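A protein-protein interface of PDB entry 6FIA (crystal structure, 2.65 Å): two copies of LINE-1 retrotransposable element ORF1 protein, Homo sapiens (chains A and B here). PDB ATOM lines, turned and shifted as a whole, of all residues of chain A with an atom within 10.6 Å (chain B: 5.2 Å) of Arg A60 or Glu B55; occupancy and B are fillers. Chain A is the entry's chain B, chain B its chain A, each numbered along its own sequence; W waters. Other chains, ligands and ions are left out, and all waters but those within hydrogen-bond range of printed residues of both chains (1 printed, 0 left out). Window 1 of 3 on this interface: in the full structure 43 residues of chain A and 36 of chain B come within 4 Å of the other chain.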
ATOM      1  N   ALA A  49      13.938  -3.394  13.428  1.00  0.00           N
ATOM      2  CA  ALA A  49      13.141  -2.886  12.309  1.00  0.00           C
ATOM      3  C   ALA A  49      13.504  -3.599  11.003  1.00  0.00           C
ATOM      4  O   ALA A  49      12.633  -3.812  10.150  1.00  0.00           O
ATOM      5  CB  ALA A  49      13.355  -1.395  12.158  1.00  0.00           C
ATOM      6  N   ARG A  50      14.791  -3.975  10.854  1.00  0.00           N
ATOM      7  CA  ARG A  50      15.295  -4.711   9.691  1.00  0.00           C
ATOM      8  C   ARG A  50      14.705  -6.126   9.669  1.00  0.00           C
ATOM      9  O   ARG A  50      14.311  -6.617   8.597  1.00  0.00           O
ATOM     10  CB  ARG A  50      16.825  -4.769   9.718  1.00  0.00           C
ATOM     11  CG  ARG A  50      17.468  -4.815   8.325  1.00  0.00           C
ATOM     12  CD  ARG A  50      17.182  -3.542   7.496  1.00  0.00           C
ATOM     13  NE  ARG A  50      17.769  -3.565   6.145  1.00  0.00           N
ATOM     14  CZ  ARG A  50      17.071  -3.744   5.020  1.00  0.00           C
ATOM     15  NH1 ARG A  50      15.755  -3.941   5.068  1.00  0.00           N
ATOM     16  NH2 ARG A  50      17.687  -3.746   3.842  1.00  0.00           N
ATOM     17  N   GLU A  51      14.621  -6.765  10.865  1.00  0.00           N
ATOM     18  CA  GLU A  51      14.047  -8.099  11.074  1.00  0.00           C
ATOM     19  C   GLU A  51      12.569  -8.094  10.733  1.00  0.00           C
ATOM     20  O   GLU A  51      12.105  -8.994  10.037  1.00  0.00           O
ATOM     21  CB  GLU A  51      14.246  -8.555  12.526  1.00  0.00           C
ATOM     22  CG  GLU A  51      15.658  -9.023  12.833  1.00  0.00           C
ATOM     23  CD  GLU A  51      16.046  -9.092  14.305  1.00  0.00           C
ATOM     24  OE1 GLU A  51      15.147  -9.027  15.177  1.00  0.00           O
ATOM     25  OE2 GLU A  51      17.261  -9.227  14.582  1.00  0.00           O
ATOM     26  N   LEU A  52      11.833  -7.051  11.193  1.00  0.00           N
ATOM     27  CA  LEU A  52      10.398  -6.892  10.927  1.00  0.00           C
ATOM     28  C   LEU A  52      10.099  -6.660   9.446  1.00  0.00           C
ATOM     29  O   LEU A  52       9.075  -7.128   8.947  1.00  0.00           O
ATOM     30  CB  LEU A  52       9.809  -5.763  11.777  1.00  0.00           C
ATOM     31  CG  LEU A  52       9.638  -6.074  13.264  1.00  0.00           C
ATOM     32  CD1 LEU A  52       9.403  -4.803  14.049  1.00  0.00           C
ATOM     33  CD2 LEU A  52       8.527  -7.112  13.517  1.00  0.00           C
ATOM     34  N   ARG A  53      11.004  -5.952   8.743  1.00  0.00           N
ATOM     35  CA  ARG A  53      10.875  -5.698   7.308  1.00  0.00           C
ATOM     36  C   ARG A  53      10.904  -7.035   6.551  1.00  0.00           C
ATOM     37  O   ARG A  53      10.067  -7.270   5.668  1.00  0.00           O
ATOM     38  CB  ARG A  53      11.995  -4.750   6.825  1.00  0.00           C
ATOM     39  CG  ARG A  53      11.803  -4.280   5.389  1.00  0.00           C
ATOM     40  CD  ARG A  53      12.476  -2.960   5.081  1.00  0.00           C
ATOM     41  NE  ARG A  53      12.564  -2.726   3.631  1.00  0.00           N
ATOM     42  CZ  ARG A  53      11.588  -2.201   2.881  1.00  0.00           C
ATOM     43  NH1 ARG A  53      10.427  -1.855   3.433  1.00  0.00           N
ATOM     44  NH2 ARG A  53      11.763  -2.032   1.575  1.00  0.00           N
ATOM     45  N   GLU A  54      11.835  -7.927   6.954  1.00  0.00           N
ATOM     46  CA  GLU A  54      12.037  -9.251   6.382  1.00  0.00           C
ATOM     47  C   GLU A  54      10.881 -10.181   6.723  1.00  0.00           C
ATOM     48  O   GLU A  54      10.453 -10.956   5.866  1.00  0.00           O
ATOM     49  CB  GLU A  54      13.392  -9.829   6.850  1.00  0.00           C
ATOM     50  CG  GLU A  54      13.793 -11.176   6.254  1.00  0.00           C
ATOM     51  CD  GLU A  54      13.751 -11.289   4.739  1.00  0.00           C
ATOM     52  OE1 GLU A  54      14.403 -10.463   4.055  1.00  0.00           O
ATOM     53  OE2 GLU A  54      13.068 -12.214   4.238  1.00  0.00           O
ATOM     54  N   GLU A  55      10.352 -10.082   7.961  1.00  0.00           N
ATOM     55  CA  GLU A  55       9.212 -10.864   8.425  1.00  0.00           C
ATOM     56  C   GLU A  55       7.996 -10.590   7.556  1.00  0.00           C
ATOM     57  O   GLU A  55       7.294 -11.536   7.180  1.00  0.00           O
ATOM     58  CB  GLU A  55       8.914 -10.572   9.898  1.00  0.00           C
ATOM     59  CG  GLU A  55       9.621 -11.521  10.852  1.00  0.00           C
ATOM     60  CD  GLU A  55       9.633 -11.115  12.316  1.00  0.00           C
ATOM     61  OE1 GLU A  55      10.741 -10.975  12.884  1.00  0.00           O
ATOM     62  OE2 GLU A  55       8.536 -11.005  12.911  1.00  0.00           O
ATOM     63  N   CYS A  56       7.771  -9.297   7.185  1.00  0.00           N
ATOM     64  CA  CYS A  56       6.661  -8.876   6.309  1.00  0.00           C
ATOM     65  C   CYS A  56       6.869  -9.312   4.863  1.00  0.00           C
ATOM     66  O   CYS A  56       5.900  -9.657   4.178  1.00  0.00           O
ATOM     67  CB  CYS A  56       6.439  -7.377   6.408  1.00  0.00           C
ATOM     68  SG  CYS A  56       5.807  -6.838   8.010  1.00  0.00           S
ATOM     69  N   ARG A  57       8.129  -9.267   4.394  1.00  0.00           N
ATOM     70  CA  ARG A  57       8.514  -9.672   3.045  1.00  0.00           C
ATOM     71  C   ARG A  57       8.180 -11.174   2.857  1.00  0.00           C
ATOM     72  O   ARG A  57       7.619 -11.561   1.829  1.00  0.00           O
ATOM     73  CB  ARG A  57      10.021  -9.390   2.829  1.00  0.00           C
ATOM     74  CG  ARG A  57      10.493  -9.542   1.380  1.00  0.00           C
ATOM     75  CD  ARG A  57      11.747 -10.421   1.230  1.00  0.00           C
ATOM     76  NE  ARG A  57      11.540 -11.799   1.709  1.00  0.00           N
ATOM     77  CZ  ARG A  57      11.283 -12.845   0.926  1.00  0.00           C
ATOM     78  NH1 ARG A  57      11.221 -12.698  -0.391  1.00  0.00           N
ATOM     79  NH2 ARG A  57      11.105 -14.051   1.454  1.00  0.00           N
ATOM     80  N   SER A  58       8.476 -11.990   3.897  1.00  0.00           N
ATOM     81  CA  SER A  58       8.212 -13.424   3.942  1.00  0.00           C
ATOM     82  C   SER A  58       6.702 -13.719   3.930  1.00  0.00           C
ATOM     83  O   SER A  58       6.260 -14.596   3.179  1.00  0.00           O
ATOM     84  CB  SER A  58       8.865 -14.047   5.173  1.00  0.00           C
ATOM     85  OG  SER A  58       8.239 -15.272   5.538  1.00  0.00           O
ATOM     86  N   LEU A  59       5.915 -12.993   4.770  1.00  0.00           N
ATOM     87  CA  LEU A  59       4.460 -13.149   4.858  1.00  0.00           C
ATOM     88  C   LEU A  59       3.763 -12.763   3.558  1.00  0.00           C
ATOM     89  O   LEU A  59       2.789 -13.399   3.173  1.00  0.00           O
ATOM     90  CB  LEU A  59       3.910 -12.323   6.018  1.00  0.00           C
ATOM     91  CG  LEU A  59       4.215 -12.869   7.411  1.00  0.00           C
ATOM     92  CD1 LEU A  59       4.082 -11.780   8.456  1.00  0.00           C
ATOM     93  CD2 LEU A  59       3.307 -14.074   7.759  1.00  0.00           C
ATOM     94  N   ARG A  60       4.283 -11.736   2.854  1.00  0.00           N
ATOM     95  CA  ARG A  60       3.732 -11.341   1.559  1.00  0.00           C
ATOM     96  C   ARG A  60       3.917 -12.433   0.515  1.00  0.00           C
ATOM     97  O   ARG A  60       2.983 -12.714  -0.225  1.00  0.00           O
ATOM     98  CB  ARG A  60       4.320 -10.031   1.090  1.00  0.00           C
ATOM     99  CG  ARG A  60       3.577  -8.826   1.640  1.00  0.00           C
ATOM    100  CD  ARG A  60       3.974  -7.548   0.925  1.00  0.00           C
ATOM    101  NE  ARG A  60       5.432  -7.392   0.818  1.00  0.00           N
ATOM    102  CZ  ARG A  60       6.188  -6.770   1.721  1.00  0.00           C
ATOM    103  NH1 ARG A  60       5.637  -6.235   2.804  1.00  0.00           N
ATOM    104  NH2 ARG A  60       7.501  -6.684   1.549  1.00  0.00           N
ATOM    105  N   SER A  61       5.085 -13.106   0.501  1.00  0.00           N
ATOM    106  CA  SER A  61       5.317 -14.194  -0.452  1.00  0.00           C
ATOM    107  C   SER A  61       4.451 -15.445  -0.115  1.00  0.00           C
ATOM    108  O   SER A  61       3.951 -16.103  -1.026  1.00  0.00           O
ATOM    109  CB  SER A  61       6.808 -14.519  -0.568  1.00  0.00           C
ATOM    110  OG  SER A  61       7.243 -15.392   0.456  1.00  0.00           O
ATOM    111  N   ARG A  62       4.210 -15.695   1.193  1.00  0.00           N
ATOM    112  CA  ARG A  62       3.330 -16.769   1.665  1.00  0.00           C
ATOM    113  C   ARG A  62       1.890 -16.530   1.210  1.00  0.00           C
ATOM    114  O   ARG A  62       1.223 -17.469   0.765  1.00  0.00           O
ATOM    115  CB  ARG A  62       3.406 -16.914   3.194  1.00  0.00           C
ATOM    116  CG  ARG A  62       4.676 -17.624   3.663  1.00  0.00           C
ATOM    117  CD  ARG A  62       4.789 -17.667   5.174  1.00  0.00           C
ATOM    118  NE  ARG A  62       3.937 -18.715   5.735  1.00  0.00           N
ATOM    119  CZ  ARG A  62       3.952 -19.106   7.007  1.00  0.00           C
ATOM    120  NH1 ARG A  62       4.765 -18.527   7.877  1.00  0.00           N
ATOM    121  NH2 ARG A  62       3.152 -20.079   7.415  1.00  0.00           N
ATOM    122  N   CYS A  63       1.427 -15.263   1.273  1.00  0.00           N
ATOM    123  CA  CYS A  63       0.088 -14.885   0.784  1.00  0.00           C
ATOM    124  C   CYS A  63      -0.016 -15.006  -0.731  1.00  0.00           C
ATOM    125  O   CYS A  63      -1.045 -15.463  -1.218  1.00  0.00           O
ATOM    126  CB  CYS A  63      -0.297 -13.490   1.251  1.00  0.00           C
ATOM    127  SG  CYS A  63      -0.638 -13.376   3.014  1.00  0.00           S
ATOM    128  N   ASP A  64       1.053 -14.605  -1.482  1.00  0.00           N
ATOM    129  CA  ASP A  64       1.099 -14.712  -2.944  1.00  0.00           C
ATOM    130  C   ASP A  64       0.859 -16.134  -3.354  1.00  0.00           C
ATOM    131  O   ASP A  64      -0.022 -16.396  -4.160  1.00  0.00           O
ATOM    132  CB  ASP A  64       2.465 -14.257  -3.487  1.00  0.00           C
ATOM    133  CG  ASP A  64       2.763 -12.771  -3.345  1.00  0.00           C
ATOM    134  OD1 ASP A  64       1.838 -11.952  -3.569  1.00  0.00           O
ATOM    135  OD2 ASP A  64       3.932 -12.425  -3.070  1.00  0.00           O
ATOM    136  N   GLN A  65       1.586 -17.067  -2.729  1.00  0.00           N
ATOM    137  CA  GLN A  65       1.489 -18.502  -2.965  1.00  0.00           C
ATOM    138  C   GLN A  65       0.118 -19.072  -2.593  1.00  0.00           C
ATOM    139  O   GLN A  65      -0.452 -19.835  -3.368  1.00  0.00           O
ATOM    140  CB  GLN A  65       2.589 -19.215  -2.196  1.00  0.00           C
ATOM    141  CG  GLN A  65       3.572 -19.937  -3.096  1.00  0.00           C
ATOM    142  CD  GLN A  65       4.123 -21.171  -2.417  1.00  0.00           C
ATOM    143  OE1 GLN A  65       5.163 -21.120  -1.751  1.00  0.00           O
ATOM    144  NE2 GLN A  65       3.414 -22.304  -2.533  1.00  0.00           N
ATOM    145  N   LEU A  66      -0.420 -18.691  -1.422  1.00  0.00           N
ATOM    146  CA  LEU A  66      -1.751 -19.121  -0.995  1.00  0.00           C
ATOM    147  C   LEU A  66      -2.834 -18.656  -1.956  1.00  0.00           C
ATOM    148  O   LEU A  66      -3.712 -19.437  -2.304  1.00  0.00           O
ATOM    149  CB  LEU A  66      -2.075 -18.637   0.435  1.00  0.00           C
ATOM    150  CG  LEU A  66      -1.448 -19.445   1.588  1.00  0.00           C
ATOM    151  CD1 LEU A  66      -1.488 -18.681   2.864  1.00  0.00           C
ATOM    152  CD2 LEU A  66      -2.128 -20.764   1.762  1.00  0.00           C
ATOM    153  N   GLU A  67      -2.763 -17.411  -2.422  1.00  0.00           N
ATOM    154  CA  GLU A  67      -3.754 -16.884  -3.360  1.00  0.00           C
ATOM    155  C   GLU A  67      -3.781 -17.672  -4.676  1.00  0.00           C
ATOM    156  O   GLU A  67      -4.865 -18.045  -5.141  1.00  0.00           O
ATOM    157  CB  GLU A  67      -3.550 -15.385  -3.573  1.00  0.00           C
ATOM    158  CG  GLU A  67      -3.928 -14.575  -2.340  1.00  0.00           C
ATOM    159  CD  GLU A  67      -3.300 -13.200  -2.184  1.00  0.00           C
ATOM    160  OE1 GLU A  67      -2.639 -12.721  -3.135  1.00  0.00           O
ATOM    161  OE2 GLU A  67      -3.508 -12.584  -1.111  1.00  0.00           O
ATOM    162  N   GLU A  68      -2.583 -18.028  -5.215  1.00  0.00           N
ATOM    163  CA  GLU A  68      -2.458 -18.849  -6.436  1.00  0.00           C
ATOM    164  C   GLU A  68      -3.103 -20.222  -6.194  1.00  0.00           C
ATOM    165  O   GLU A  68      -3.911 -20.672  -7.006  1.00  0.00           O
ATOM    166  CB  GLU A  68      -0.979 -19.062  -6.828  1.00  0.00           C
ATOM    167  CG  GLU A  68      -0.205 -17.818  -7.241  1.00  0.00           C
ATOM    168  CD  GLU A  68       1.312 -17.976  -7.229  1.00  0.00           C
ATOM    169  OE1 GLU A  68       1.799 -19.129  -7.307  1.00  0.00           O
ATOM    170  OE2 GLU A  68       2.015 -16.941  -7.140  1.00  0.00           O
ATOM    171  N   GLU B  51       5.352   2.524   8.289  1.00  0.00           N
ATOM    172  CA  GLU B  51       5.309   1.704   7.077  1.00  0.00           C
ATOM    173  C   GLU B  51       5.019   0.264   7.422  1.00  0.00           C
ATOM    174  O   GLU B  51       4.168  -0.352   6.778  1.00  0.00           O
ATOM    175  CB  GLU B  51       6.638   1.801   6.297  1.00  0.00           C
ATOM    176  CG  GLU B  51       6.812   3.102   5.528  1.00  0.00           C
ATOM    177  CD  GLU B  51       8.229   3.465   5.107  1.00  0.00           C
ATOM    178  OE1 GLU B  51       9.123   2.587   5.165  1.00  0.00           O
ATOM    179  OE2 GLU B  51       8.435   4.629   4.691  1.00  0.00           O
ATOM    180  N   LEU B  52       5.706  -0.271   8.457  1.00  0.00           N
ATOM    181  CA  LEU B  52       5.517  -1.658   8.932  1.00  0.00           C
ATOM    182  C   LEU B  52       4.134  -1.882   9.505  1.00  0.00           C
ATOM    183  O   LEU B  52       3.587  -2.965   9.348  1.00  0.00           O
ATOM    184  CB  LEU B  52       6.585  -2.051   9.956  1.00  0.00           C
ATOM    185  CG  LEU B  52       8.002  -2.248   9.409  1.00  0.00           C
ATOM    186  CD1 LEU B  52       9.014  -2.278  10.529  1.00  0.00           C
ATOM    187  CD2 LEU B  52       8.108  -3.501   8.543  1.00  0.00           C
ATOM    188  N   ARG B  53       3.562  -0.857  10.170  1.00  0.00           N
ATOM    189  CA  ARG B  53       2.215  -0.929  10.737  1.00  0.00           C
ATOM    190  C   ARG B  53       1.194  -1.132   9.596  1.00  0.00           C
ATOM    191  O   ARG B  53       0.298  -1.994   9.696  1.00  0.00           O
ATOM    192  CB  ARG B  53       1.929   0.343  11.546  1.00  0.00           C
ATOM    193  CG  ARG B  53       0.649   0.324  12.388  1.00  0.00           C
ATOM    194  CD  ARG B  53       0.529   1.605  13.240  1.00  0.00           C
ATOM    195  NE  ARG B  53      -0.809   2.216  13.175  1.00  0.00           N
ATOM    196  CZ  ARG B  53      -1.046   3.510  12.950  1.00  0.00           C
ATOM    197  NH1 ARG B  53      -0.036   4.358  12.761  1.00  0.00           N
ATOM    198  NH2 ARG B  53      -2.291   3.964  12.901  1.00  0.00           N
ATOM    199  N   GLU B  54       1.382  -0.387   8.493  1.00  0.00           N
ATOM    200  CA  GLU B  54       0.532  -0.426   7.311  1.00  0.00           C
ATOM    201  C   GLU B  54       0.728  -1.745   6.534  1.00  0.00           C
ATOM    202  O   GLU B  54      -0.250  -2.316   6.040  1.00  0.00           O
ATOM    203  CB  GLU B  54       0.801   0.818   6.443  1.00  0.00           C
ATOM    204  CG  GLU B  54      -0.045   0.947   5.191  1.00  0.00           C
ATOM    205  CD  GLU B  54      -1.547   0.838   5.365  1.00  0.00           C
ATOM    206  OE1 GLU B  54      -2.118   1.613   6.171  1.00  0.00           O
ATOM    207  OE2 GLU B  54      -2.157  -0.007   4.667  1.00  0.00           O
ATOM    208  N   GLU B  55       1.979  -2.244   6.473  1.00  0.00           N
ATOM    209  CA  GLU B  55       2.308  -3.517   5.845  1.00  0.00           C
ATOM    210  C   GLU B  55       1.536  -4.668   6.521  1.00  0.00           C
ATOM    211  O   GLU B  55       1.013  -5.528   5.825  1.00  0.00           O
ATOM    212  CB  GLU B  55       3.826  -3.775   5.896  1.00  0.00           C
ATOM    213  CG  GLU B  55       4.576  -3.302   4.664  1.00  0.00           C
ATOM    214  CD  GLU B  55       6.095  -3.267   4.773  1.00  0.00           C
ATOM    215  OE1 GLU B  55       6.702  -4.337   5.014  1.00  0.00           O
ATOM    216  OE2 GLU B  55       6.684  -2.186   4.534  1.00  0.00           O
ATOM    217  N   CYS B  56       1.437  -4.647   7.873  1.00  0.00           N
ATOM    218  CA  CYS B  56       0.702  -5.643   8.679  1.00  0.00           C
ATOM    219  C   CYS B  56      -0.791  -5.501   8.491  1.00  0.00           C
ATOM    220  O   CYS B  56      -1.497  -6.497   8.535  1.00  0.00           O
ATOM    221  CB  CYS B  56       1.070  -5.537  10.159  1.00  0.00           C
ATOM    222  SG  CYS B  56       2.743  -6.089  10.566  1.00  0.00           S
ATOM    223  N   ARG B  57      -1.286  -4.256   8.389  1.00  0.00           N
ATOM    224  CA  ARG B  57      -2.705  -3.959   8.200  1.00  0.00           C
ATOM    225  C   ARG B  57      -3.171  -4.591   6.858  1.00  0.00           C
ATOM    226  O   ARG B  57      -4.222  -5.261   6.802  1.00  0.00           O
ATOM    227  CB  ARG B  57      -2.922  -2.432   8.221  1.00  0.00           C
ATOM    228  CG  ARG B  57      -4.394  -2.001   8.265  1.00  0.00           C
ATOM    229  CD  ARG B  57      -4.764  -0.952   7.202  1.00  0.00           C
ATOM    230  NE  ARG B  57      -4.567  -1.437   5.823  1.00  0.00           N
ATOM    231  CZ  ARG B  57      -5.527  -1.945   5.051  1.00  0.00           C
ATOM    232  NH1 ARG B  57      -5.246  -2.362   3.822  1.00  0.00           N
ATOM    233  NH2 ARG B  57      -6.771  -2.051   5.506  1.00  0.00           N
ATOM    234  N   SER B  58      -2.328  -4.444   5.807  1.00  0.00           N
ATOM    235  CA  SER B  58      -2.547  -5.013   4.477  1.00  0.00           C
ATOM    236  C   SER B  58      -2.565  -6.560   4.521  1.00  0.00           C
ATOM    237  O   SER B  58      -3.463  -7.170   3.943  1.00  0.00           O
ATOM    238  CB  SER B  58      -1.481  -4.511   3.503  1.00  0.00           C
ATOM    239  OG  SER B  58      -1.333  -5.391   2.394  1.00  0.00           O
ATOM    240  N   LEU B  59      -1.578  -7.181   5.212  1.00  0.00           N
ATOM    241  CA  LEU B  59      -1.483  -8.637   5.357  1.00  0.00           C
ATOM    242  C   LEU B  59      -2.639  -9.205   6.163  1.00  0.00           C
ATOM    243  O   LEU B  59      -3.118 -10.285   5.847  1.00  0.00           O
ATOM    244  CB  LEU B  59      -0.144  -9.060   5.973  1.00  0.00           C
ATOM    245  CG  LEU B  59       1.092  -9.020   5.057  1.00  0.00           C
ATOM    246  CD1 LEU B  59       2.329  -8.777   5.856  1.00  0.00           C
ATOM    247  CD2 LEU B  59       1.255 -10.312   4.310  1.00  0.00           C
ATOM    248  N   ARG B  62      -5.522  -9.449   3.736  1.00  0.00           N
ATOM    249  CA  ARG B  62      -5.241 -10.521   2.779  1.00  0.00           C
ATOM    250  C   ARG B  62      -5.555 -11.877   3.404  1.00  0.00           C
ATOM    251  O   ARG B  62      -6.141 -12.740   2.746  1.00  0.00           O
ATOM    252  CB  ARG B  62      -3.778 -10.467   2.320  1.00  0.00           C
ATOM    253  CG  ARG B  62      -3.497  -9.353   1.311  1.00  0.00           C
ATOM    254  CD  ARG B  62      -2.057  -9.337   0.916  1.00  0.00           C
ATOM    255  NE  ARG B  62      -1.742 -10.369  -0.070  1.00  0.00           N
ATOM    256  CZ  ARG B  62      -0.533 -10.572  -0.578  1.00  0.00           C
ATOM    257  NH1 ARG B  62       0.492  -9.829  -0.185  1.00  0.00           N
ATOM    258  NH2 ARG B  62      -0.334 -11.539  -1.470  1.00  0.00           N
HETATM  259  O   HOH W   1      -6.154 -12.069  -0.137  1.00  0.00           O
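Of the printed residues of chain B, Ala A49 touches Leu B52. Printed residues of chain B within 4 Å of Leu A52: Leu B52 (3.8 Å). Of chain B, only Glu B55, Leu B59 and Arg B62 come within 4 Å of Arg A60. Of the printed residues of chain B, Glu A67 touches Arg B62. Of chain A, only Ala A49 (3.9 Å), Leu A52 (3.8 Å) and Arg A53 (3.7 Å) come within 4 Å of Leu B52. No residue of chain A comes within 4 Å of Glu B54. Of chain A, only Arg A53 (3.9 Å), Cys A56 (3.4 Å) and Arg A60 (3.1 Å) come within 4 Å of Glu B55. No residue of chain A comes within 4 Å of Ser B58. Of chain A, only Leu A59, Arg A60 and Cys A63 come within 4 Å of Leu B59. The nearest printed residue of chain B that does not touch Arg A60 is Ser B58 (5.9 Å).
The side-chain sulfur of Cys A63 lies within hydrogen-bond range of the backbone carbonyl oxygen of Leu A59 (3.4 Å). SG of Cys A56 is in hydrogen-bond range of O of Leu A52. The side-chain sulfur (SG) of Cys B56 is in hydrogen-bond range of the backbone carbonyl oxygen (O) of Leu B52.
Water W1 lies within hydrogen-bond range of the side-chain carboxylate (OE2) of Glu A67 (2.9 Å) and the backbone carbonyl oxygen (O) of Arg B62 (3.0 Å).
The guanidinium group of Arg B62 lies within salt-bridge range of the side-chain carboxylate of Asp A64 (3.0 Å). The side-chain carboxylate (OE1) of Glu B55 is in salt-bridge range of the guanidinium group (NH1) of Arg A60 (3.1 Å). NE of Arg B62 is in salt-bridge range of OE2 of Glu A67, 3.0 Å away. OE2 of Glu B55 lies within salt-bridge range of NH1 of Arg A53, 3.9 Å away.
Of the 10 printed residues of chain B, 4 touch a printed residue of chain A. Hydrophobic or aromatic side chains of chain B within 4 Å of the printed part of chain A: Leu B52 and Leu B59. Of the 20 printed residues of chain A, 9 touch a printed residue of chain B. Hydrophobic or aromatic side chains of chain A that line the printed part of chain B: Leu A52 and Leu A59. Along chain A the printed residues that touch a printed residue of chain B span positions 49 to 67. Among the printed residues, Asp or Glu carboxylates within 4 Å of a Lys or Arg side-chain nitrogen of the other chain: Arg A53 with Glu B55, Arg A60 with Glu B55, Asp A64 with Arg B62 and Glu A67 with Arg B62.
Among the printed residues, merely in contact across the chains: Cys A63 with Arg B62, Cys A56 with Glu B55, Leu A59 with Leu B59, Arg A60 with Leu B59, Arg A60 with Arg B62, Arg A53 with Leu B52, Leu A52 with Leu B52, Cys A63 with Leu B59 and Ala A49 with Leu B52.
Leu B52 touches its own counterpart, Leu A52. Arg A53 touches Leu B52, but with the chains exchanged Leu A52 does not touch Arg B53 (8.0 Å). Arg A53 touches Glu B55, but with the chains exchanged Glu A55 does not touch Arg B53 (11.0 Å). Leu B59 touches its own counterpart, Leu A59. 10 positions are printed for both chains. Of the 13 pairs that touch across the chains among the printed residues, 2 have their exchanged pair printed and touching as well.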
